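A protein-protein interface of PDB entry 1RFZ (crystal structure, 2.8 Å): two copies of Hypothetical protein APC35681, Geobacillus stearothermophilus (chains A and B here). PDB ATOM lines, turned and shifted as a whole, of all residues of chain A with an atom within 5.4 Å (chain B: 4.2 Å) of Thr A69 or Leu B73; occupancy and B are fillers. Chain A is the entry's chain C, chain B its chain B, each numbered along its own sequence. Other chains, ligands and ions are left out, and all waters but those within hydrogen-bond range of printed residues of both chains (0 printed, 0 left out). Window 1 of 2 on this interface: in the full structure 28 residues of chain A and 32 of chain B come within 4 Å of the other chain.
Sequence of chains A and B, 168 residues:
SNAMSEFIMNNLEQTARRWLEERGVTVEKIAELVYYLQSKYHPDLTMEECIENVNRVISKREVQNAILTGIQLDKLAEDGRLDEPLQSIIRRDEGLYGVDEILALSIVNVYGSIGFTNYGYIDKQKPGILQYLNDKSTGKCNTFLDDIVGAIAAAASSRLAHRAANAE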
ATOM      1  N   TRP A  19     -24.335  17.409  -6.776  1.00  0.00           N
ATOM      2  CA  TRP A  19     -23.117  16.681  -6.408  1.00  0.00           C
ATOM      3  C   TRP A  19     -23.450  15.248  -6.005  1.00  0.00           C
ATOM      4  O   TRP A  19     -22.715  14.327  -6.357  1.00  0.00           O
ATOM      5  CB  TRP A  19     -22.379  17.397  -5.265  1.00  0.00           C
ATOM      6  CG  TRP A  19     -21.631  18.616  -5.716  1.00  0.00           C
ATOM      7  CD1 TRP A  19     -22.045  19.544  -6.638  1.00  0.00           C
ATOM      8  CD2 TRP A  19     -20.368  19.082  -5.223  1.00  0.00           C
ATOM      9  NE1 TRP A  19     -21.122  20.554  -6.746  1.00  0.00           N
ATOM     10  CE2 TRP A  19     -20.082  20.300  -5.889  1.00  0.00           C
ATOM     11  CE3 TRP A  19     -19.451  18.596  -4.278  1.00  0.00           C
ATOM     12  CZ2 TRP A  19     -18.921  21.033  -5.642  1.00  0.00           C
ATOM     13  CZ3 TRP A  19     -18.297  19.331  -4.033  1.00  0.00           C
ATOM     14  CH2 TRP A  19     -18.045  20.535  -4.714  1.00  0.00           C
ATOM     15  N   GLN A  64     -25.466  20.631   3.762  1.00  0.00           N
ATOM     16  CA  GLN A  64     -24.844  20.953   2.489  1.00  0.00           C
ATOM     17  C   GLN A  64     -23.330  21.029   2.612  1.00  0.00           C
ATOM     18  O   GLN A  64     -22.612  20.388   1.843  1.00  0.00           O
ATOM     19  CB  GLN A  64     -25.385  22.266   1.971  1.00  0.00           C
ATOM     20  CG  GLN A  64     -26.724  22.130   1.334  1.00  0.00           C
ATOM     21  CD  GLN A  64     -27.573  23.336   1.557  1.00  0.00           C
ATOM     22  OE1 GLN A  64     -27.102  24.466   1.438  1.00  0.00           O
ATOM     23  NE2 GLN A  64     -28.843  23.114   1.886  1.00  0.00           N
ATOM     24  N   ASN A  65     -22.855  21.804   3.590  1.00  0.00           N
ATOM     25  CA  ASN A  65     -21.431  21.964   3.842  1.00  0.00           C
ATOM     26  C   ASN A  65     -20.696  20.629   3.938  1.00  0.00           C
ATOM     27  O   ASN A  65     -19.621  20.446   3.364  1.00  0.00           O
ATOM     28  CB  ASN A  65     -21.207  22.729   5.145  1.00  0.00           C
ATOM     29  CG  ASN A  65     -21.545  24.194   5.031  1.00  0.00           C
ATOM     30  OD1 ASN A  65     -21.517  24.780   3.943  1.00  0.00           O
ATOM     31  ND2 ASN A  65     -21.845  24.809   6.167  1.00  0.00           N
ATOM     32  N   ALA A  66     -21.278  19.696   4.682  1.00  0.00           N
ATOM     33  CA  ALA A  66     -20.691  18.381   4.869  1.00  0.00           C
ATOM     34  C   ALA A  66     -20.615  17.622   3.536  1.00  0.00           C
ATOM     35  O   ALA A  66     -19.591  17.033   3.211  1.00  0.00           O
ATOM     36  CB  ALA A  66     -21.529  17.618   5.852  1.00  0.00           C
ATOM     37  N   ILE A  67     -21.711  17.639   2.784  1.00  0.00           N
ATOM     38  CA  ILE A  67     -21.807  16.965   1.510  1.00  0.00           C
ATOM     39  C   ILE A  67     -20.742  17.451   0.516  1.00  0.00           C
ATOM     40  O   ILE A  67     -20.025  16.637  -0.099  1.00  0.00           O
ATOM     41  CB  ILE A  67     -23.227  17.183   0.893  1.00  0.00           C
ATOM     42  CG1 ILE A  67     -24.284  16.542   1.792  1.00  0.00           C
ATOM     43  CG2 ILE A  67     -23.308  16.612  -0.539  1.00  0.00           C
ATOM     44  CD1 ILE A  67     -25.678  16.801   1.324  1.00  0.00           C
ATOM     45  N   LEU A  68     -20.626  18.765   0.341  1.00  0.00           N
ATOM     46  CA  LEU A  68     -19.637  19.282  -0.595  1.00  0.00           C
ATOM     47  C   LEU A  68     -18.217  18.899  -0.201  1.00  0.00           C
ATOM     48  O   LEU A  68     -17.398  18.523  -1.042  1.00  0.00           O
ATOM     49  CB  LEU A  68     -19.739  20.801  -0.709  1.00  0.00           C
ATOM     50  CG  LEU A  68     -21.039  21.354  -1.299  1.00  0.00           C
ATOM     51  CD1 LEU A  68     -20.992  22.864  -1.323  1.00  0.00           C
ATOM     52  CD2 LEU A  68     -21.225  20.842  -2.698  1.00  0.00           C
ATOM     53  N   THR A  69     -17.923  18.965   1.084  1.00  0.00           N
ATOM     54  CA  THR A  69     -16.580  18.658   1.517  1.00  0.00           C
ATOM     55  C   THR A  69     -16.254  17.182   1.361  1.00  0.00           C
ATOM     56  O   THR A  69     -15.211  16.810   0.796  1.00  0.00           O
ATOM     57  CB  THR A  69     -16.368  19.083   2.988  1.00  0.00           C
ATOM     58  OG1 THR A  69     -16.957  20.373   3.203  1.00  0.00           O
ATOM     59  CG2 THR A  69     -14.881  19.168   3.298  1.00  0.00           C
ATOM     60  N   GLY A  70     -17.155  16.347   1.865  1.00  0.00           N
ATOM     61  CA  GLY A  70     -16.966  14.910   1.803  1.00  0.00           C
ATOM     62  C   GLY A  70     -16.802  14.397   0.392  1.00  0.00           C
ATOM     63  O   GLY A  70     -15.866  13.652   0.101  1.00  0.00           O
ATOM     64  N   ILE A  71     -17.711  14.802  -0.489  1.00  0.00           N
ATOM     65  CA  ILE A  71     -17.656  14.379  -1.880  1.00  0.00           C
ATOM     66  C   ILE A  71     -16.361  14.855  -2.539  1.00  0.00           C
ATOM     67  O   ILE A  71     -15.659  14.056  -3.187  1.00  0.00           O
ATOM     68  CB  ILE A  71     -18.878  14.903  -2.644  1.00  0.00           C
ATOM     69  CG1 ILE A  71     -20.099  14.050  -2.268  1.00  0.00           C
ATOM     70  CG2 ILE A  71     -18.584  14.930  -4.140  1.00  0.00           C
ATOM     71  CD1 ILE A  71     -21.396  14.602  -2.756  1.00  0.00           C
ATOM     72  N   GLN A  72     -16.052  16.143  -2.351  1.00  0.00           N
ATOM     73  CA  GLN A  72     -14.840  16.774  -2.881  1.00  0.00           C
ATOM     74  C   GLN A  72     -13.588  15.913  -2.620  1.00  0.00           C
ATOM     75  O   GLN A  72     -12.801  15.645  -3.540  1.00  0.00           O
ATOM     76  CB  GLN A  72     -14.654  18.163  -2.237  1.00  0.00           C
ATOM     77  CG  GLN A  72     -13.351  18.874  -2.639  1.00  0.00           C
ATOM     78  CD  GLN A  72     -13.363  19.321  -4.083  1.00  0.00           C
ATOM     79  OE1 GLN A  72     -13.858  20.406  -4.387  1.00  0.00           O
ATOM     80  NE2 GLN A  72     -12.850  18.483  -4.987  1.00  0.00           N
ATOM     81  N   LEU A  73     -13.411  15.481  -1.368  1.00  0.00           N
ATOM     82  CA  LEU A  73     -12.252  14.653  -1.003  1.00  0.00           C
ATOM     83  C   LEU A  73     -12.265  13.298  -1.718  1.00  0.00           C
ATOM     84  O   LEU A  73     -11.233  12.840  -2.226  1.00  0.00           O
ATOM     85  CB  LEU A  73     -12.201  14.469   0.524  1.00  0.00           C
ATOM     86  CG  LEU A  73     -11.903  15.788   1.255  1.00  0.00           C
ATOM     87  CD1 LEU A  73     -12.007  15.603   2.755  1.00  0.00           C
ATOM     88  CD2 LEU A  73     -10.530  16.287   0.856  1.00  0.00           C
ATOM     89  N   ASP A  74     -13.447  12.678  -1.747  1.00  0.00           N
ATOM     90  CA  ASP A  74     -13.661  11.396  -2.419  1.00  0.00           C
ATOM     91  C   ASP A  74     -13.180  11.508  -3.872  1.00  0.00           C
ATOM     92  O   ASP A  74     -12.477  10.625  -4.379  1.00  0.00           O
ATOM     93  CB  ASP A  74     -15.155  11.022  -2.416  1.00  0.00           C
ATOM     94  CG  ASP A  74     -15.612  10.375  -1.110  1.00  0.00           C
ATOM     95  OD1 ASP A  74     -14.822  10.342  -0.148  1.00  0.00           O
ATOM     96  OD2 ASP A  74     -16.770   9.902  -1.044  1.00  0.00           O
ATOM     97  N   LEU A 103     -17.736  14.180   9.771  1.00  0.00           N
ATOM     98  CA  LEU A 103     -18.656  14.921   8.917  1.00  0.00           C
ATOM     99  C   LEU A 103     -20.062  14.373   8.975  1.00  0.00           C
ATOM    100  O   LEU A 103     -21.033  15.128   8.989  1.00  0.00           O
ATOM    101  CB  LEU A 103     -18.181  14.917   7.472  1.00  0.00           C
ATOM    102  CG  LEU A 103     -17.238  16.050   7.056  1.00  0.00           C
ATOM    103  CD1 LEU A 103     -16.716  15.805   5.640  1.00  0.00           C
ATOM    104  CD2 LEU A 103     -17.993  17.376   7.087  1.00  0.00           C
ATOM    105  N   THR B  69      -6.016  16.582   7.041  1.00  0.00           N
ATOM    106  CA  THR B  69      -7.201  16.924   6.268  1.00  0.00           C
ATOM    107  C   THR B  69      -7.396  18.429   6.097  1.00  0.00           C
ATOM    108  O   THR B  69      -7.526  18.926   4.972  1.00  0.00           O
ATOM    109  CB  THR B  69      -8.482  16.317   6.918  1.00  0.00           C
ATOM    110  OG1 THR B  69      -8.297  14.910   7.150  1.00  0.00           O
ATOM    111  CG2 THR B  69      -9.691  16.511   6.003  1.00  0.00           C
ATOM    112  N   GLY B  70      -7.435  19.158   7.206  1.00  0.00           N
ATOM    113  CA  GLY B  70      -7.627  20.597   7.128  1.00  0.00           C
ATOM    114  C   GLY B  70      -6.550  21.315   6.324  1.00  0.00           C
ATOM    115  O   GLY B  70      -6.850  22.178   5.488  1.00  0.00           O
ATOM    116  N   ILE B  71      -5.288  20.985   6.568  1.00  0.00           N
ATOM    117  CA  ILE B  71      -4.231  21.638   5.807  1.00  0.00           C
ATOM    118  C   ILE B  71      -4.412  21.303   4.317  1.00  0.00           C
ATOM    119  O   ILE B  71      -4.382  22.195   3.468  1.00  0.00           O
ATOM    120  CB  ILE B  71      -2.827  21.208   6.322  1.00  0.00           C
ATOM    121  CG1 ILE B  71      -2.509  21.966   7.623  1.00  0.00           C
ATOM    122  CG2 ILE B  71      -1.772  21.479   5.271  1.00  0.00           C
ATOM    123  CD1 ILE B  71      -1.198  21.535   8.311  1.00  0.00           C
ATOM    124  N   GLN B  72      -4.628  20.023   4.010  1.00  0.00           N
ATOM    125  CA  GLN B  72      -4.842  19.585   2.636  1.00  0.00           C
ATOM    126  C   GLN B  72      -5.865  20.484   1.954  1.00  0.00           C
ATOM    127  O   GLN B  72      -5.692  20.891   0.791  1.00  0.00           O
ATOM    128  CB  GLN B  72      -5.362  18.148   2.603  1.00  0.00           C
ATOM    129  CG  GLN B  72      -5.695  17.665   1.214  1.00  0.00           C
ATOM    130  CD  GLN B  72      -4.451  17.307   0.417  1.00  0.00           C
ATOM    131  OE1 GLN B  72      -3.805  16.297   0.698  1.00  0.00           O
ATOM    132  NE2 GLN B  72      -4.106  18.128  -0.582  1.00  0.00           N
ATOM    133  N   LEU B  73      -6.935  20.793   2.685  1.00  0.00           N
ATOM    134  CA  LEU B  73      -7.988  21.634   2.139  1.00  0.00           C
ATOM    135  C   LEU B  73      -7.543  23.081   1.963  1.00  0.00           C
ATOM    136  O   LEU B  73      -7.768  23.656   0.903  1.00  0.00           O
ATOM    137  CB  LEU B  73      -9.254  21.519   3.009  1.00  0.00           C
ATOM    138  CG  LEU B  73     -10.035  20.194   2.799  1.00  0.00           C
ATOM    139  CD1 LEU B  73     -11.094  19.991   3.872  1.00  0.00           C
ATOM    140  CD2 LEU B  73     -10.653  20.199   1.392  1.00  0.00           C
ATOM    141  N   ASP B  74      -6.895  23.666   2.974  1.00  0.00           N
ATOM    142  CA  ASP B  74      -6.406  25.050   2.857  1.00  0.00           C
ATOM    143  C   ASP B  74      -5.460  25.127   1.643  1.00  0.00           C
ATOM    144  O   ASP B  74      -5.536  26.052   0.817  1.00  0.00           O
ATOM    145  CB  ASP B  74      -5.651  25.496   4.125  1.00  0.00           C
ATOM    146  CG  ASP B  74      -6.580  25.833   5.289  1.00  0.00           C
ATOM    147  OD1 ASP B  74      -7.690  26.356   5.045  1.00  0.00           O
ATOM    148  OD2 ASP B  74      -6.192  25.599   6.454  1.00  0.00           O
ATOM    149  N   LYS B  75      -4.562  24.151   1.552  1.00  0.00           N
ATOM    150  CA  LYS B  75      -3.644  24.103   0.443  1.00  0.00           C
ATOM    151  C   LYS B  75      -4.434  24.121  -0.886  1.00  0.00           C
ATOM    152  O   LYS B  75      -4.169  24.950  -1.773  1.00  0.00           O
ATOM    153  CB  LYS B  75      -2.765  22.844   0.544  1.00  0.00           C
ATOM    154  CG  LYS B  75      -1.416  23.082   1.222  1.00  0.00           C
ATOM    155  CD  LYS B  75      -0.895  21.861   1.995  1.00  0.00           C
ATOM    156  CE  LYS B  75      -0.226  20.786   1.119  1.00  0.00           C
ATOM    157  NZ  LYS B  75       0.050  19.497   1.861  1.00  0.00           N
ATOM    158  N   LEU B  76      -5.411  23.227  -1.020  1.00  0.00           N
ATOM    159  CA  LEU B  76      -6.188  23.153  -2.261  1.00  0.00           C
ATOM    160  C   LEU B  76      -6.948  24.434  -2.584  1.00  0.00           C
ATOM    161  O   LEU B  76      -6.958  24.890  -3.731  1.00  0.00           O
ATOM    162  CB  LEU B  76      -7.163  21.964  -2.226  1.00  0.00           C
ATOM    163  CG  LEU B  76      -6.519  20.575  -2.263  1.00  0.00           C
ATOM    164  CD1 LEU B  76      -7.548  19.498  -1.972  1.00  0.00           C
ATOM    165  CD2 LEU B  76      -5.874  20.376  -3.617  1.00  0.00           C
ATOM    166  N   ALA B  77      -7.592  25.007  -1.573  1.00  0.00           N
ATOM    167  CA  ALA B  77      -8.333  26.242  -1.764  1.00  0.00           C
ATOM    168  C   ALA B  77      -7.372  27.361  -2.199  1.00  0.00           C
ATOM    169  O   ALA B  77      -7.733  28.260  -2.948  1.00  0.00           O
ATOM    170  CB  ALA B  77      -9.016  26.615  -0.478  1.00  0.00           C
ATOM    171  N   LEU B  82      -9.985  23.406  -5.805  1.00  0.00           N
ATOM    172  CA  LEU B  82     -11.223  22.830  -5.285  1.00  0.00           C
ATOM    173  C   LEU B  82     -12.266  23.223  -6.296  1.00  0.00           C
ATOM    174  O   LEU B  82     -12.003  24.088  -7.122  1.00  0.00           O
ATOM    175  CB  LEU B  82     -11.610  23.457  -3.955  1.00  0.00           C
ATOM    176  CG  LEU B  82     -10.834  23.207  -2.674  1.00  0.00           C
ATOM    177  CD1 LEU B  82     -11.520  23.950  -1.545  1.00  0.00           C
ATOM    178  CD2 LEU B  82     -10.791  21.731  -2.381  1.00  0.00           C
ATOM    179  N   LEU B  86     -17.317  25.163  -3.322  1.00  0.00           N
ATOM    180  CA  LEU B  86     -16.487  24.875  -2.144  1.00  0.00           C
ATOM    181  C   LEU B  86     -15.239  25.726  -2.164  1.00  0.00           C
ATOM    182  O   LEU B  86     -14.839  26.275  -1.142  1.00  0.00           O
ATOM    183  CB  LEU B  86     -16.079  23.415  -2.080  1.00  0.00           C
ATOM    184  CG  LEU B  86     -16.240  22.709  -0.721  1.00  0.00           C
ATOM    185  CD1 LEU B  86     -15.202  21.634  -0.598  1.00  0.00           C
ATOM    186  CD2 LEU B  86     -16.083  23.669   0.404  1.00  0.00           C
ATOM    187  N   TYR B  97     -19.898  28.275   7.002  1.00  0.00           N
ATOM    188  CA  TYR B  97     -19.193  27.011   6.850  1.00  0.00           C
ATOM    189  C   TYR B  97     -18.562  26.608   8.184  1.00  0.00           C
ATOM    190  O   TYR B  97     -17.743  27.353   8.733  1.00  0.00           O
ATOM    191  CB  TYR B  97     -18.108  27.161   5.789  1.00  0.00           C
ATOM    192  CG  TYR B  97     -17.410  25.866   5.416  1.00  0.00           C
ATOM    193  CD1 TYR B  97     -18.076  24.865   4.701  1.00  0.00           C
ATOM    194  CD2 TYR B  97     -16.061  25.679   5.713  1.00  0.00           C
ATOM    195  CE1 TYR B  97     -17.416  23.725   4.284  1.00  0.00           C
ATOM    196  CE2 TYR B  97     -15.387  24.540   5.300  1.00  0.00           C
ATOM    197  CZ  TYR B  97     -16.068  23.569   4.583  1.00  0.00           C
ATOM    198  OH  TYR B  97     -15.378  22.460   4.167  1.00  0.00           O
ATOM    199  N   VAL B  99     -17.252  23.190   8.736  1.00  0.00           N
ATOM    200  CA  VAL B  99     -16.491  21.962   8.629  1.00  0.00           C
ATOM    201  C   VAL B  99     -15.122  22.124   9.289  1.00  0.00           C
ATOM    202  O   VAL B  99     -14.557  21.158   9.826  1.00  0.00           O
ATOM    203  CB  VAL B  99     -16.391  21.511   7.138  1.00  0.00           C
ATOM    204  CG1 VAL B  99     -15.481  20.279   6.999  1.00  0.00           C
ATOM    205  CG2 VAL B  99     -17.819  21.197   6.600  1.00  0.00           C
ATOM    206  N   PHE B 144      -8.845  26.314   7.630  1.00  0.00           N
ATOM    207  CA  PHE B 144      -8.860  25.175   8.535  1.00  0.00           C
ATOM    208  C   PHE B 144      -7.767  25.277   9.590  1.00  0.00           C
ATOM    209  O   PHE B 144      -8.050  25.117  10.776  1.00  0.00           O
ATOM    210  CB  PHE B 144      -8.711  23.850   7.771  1.00  0.00           C
ATOM    211  CG  PHE B 144      -9.964  23.409   7.106  1.00  0.00           C
ATOM    212  CD1 PHE B 144     -10.309  23.897   5.853  1.00  0.00           C
ATOM    213  CD2 PHE B 144     -10.848  22.568   7.770  1.00  0.00           C
ATOM    214  CE1 PHE B 144     -11.520  23.553   5.276  1.00  0.00           C
ATOM    215  CE2 PHE B 144     -12.065  22.212   7.215  1.00  0.00           C
ATOM    216  CZ  PHE B 144     -12.409  22.700   5.968  1.00  0.00           C
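OH of Tyr B97 sits at hydrogen-bond distance from OG1 of Thr A69 (2.8 Å).
The side-chain hydroxyl (OG1) of Thr A69 lies within hydrogen-bond range of the backbone carbonyl oxygen (O) of Asn A65, at 2.7 Å.
Printed residues of chain A that touch a printed residue of chain B: Asn A65, Leu A68, Thr A69, Gln A72, Leu A73 and Leu A103.
Hydrophobic or aromatic side chains of chain A that line the printed part of chain B: Leu A68, Leu A73 and Leu A103.
Thr A69 touches Leu B73, but with the chains exchanged Leu A73 does not touch Thr B69 (4.1 Å).
Leu B73 touches its own counterpart, Leu A73.
6 positions are printed for both chains.
Thr A69 touches just these residues of chain B: Leu B73, Leu B86, Tyr B97 and Val B99.
Of the printed residues of chain A, Leu B73 touches Thr A69 (3.9 Å) and Leu A73 (3.95 Å).
Of the printed residues of chain B, Gln A72 touches Leu B82 and Leu B86.
Printed residues of chain B within 4 Å of Leu A103: Val B99.
Among the printed residues, merely in contact across the chains: Asn A65 with Tyr B97 (3.5 Å), Asn A65 with Val B99 (3.8 Å), Leu A68 with Leu B86 (3.8 Å), Thr A69 with Leu B73 (3.9 Å), Thr A69 with Leu B86 (3.9 Å), Thr A69 with Val B99 (3.6 Å), Gln A72 with Leu B82 (3.7 Å), Gln A72 with Leu B86 (3.9 Å), Leu A73 with Leu B73 (3.95 Å) and Leu A103 with Val B99 (3.8 Å).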
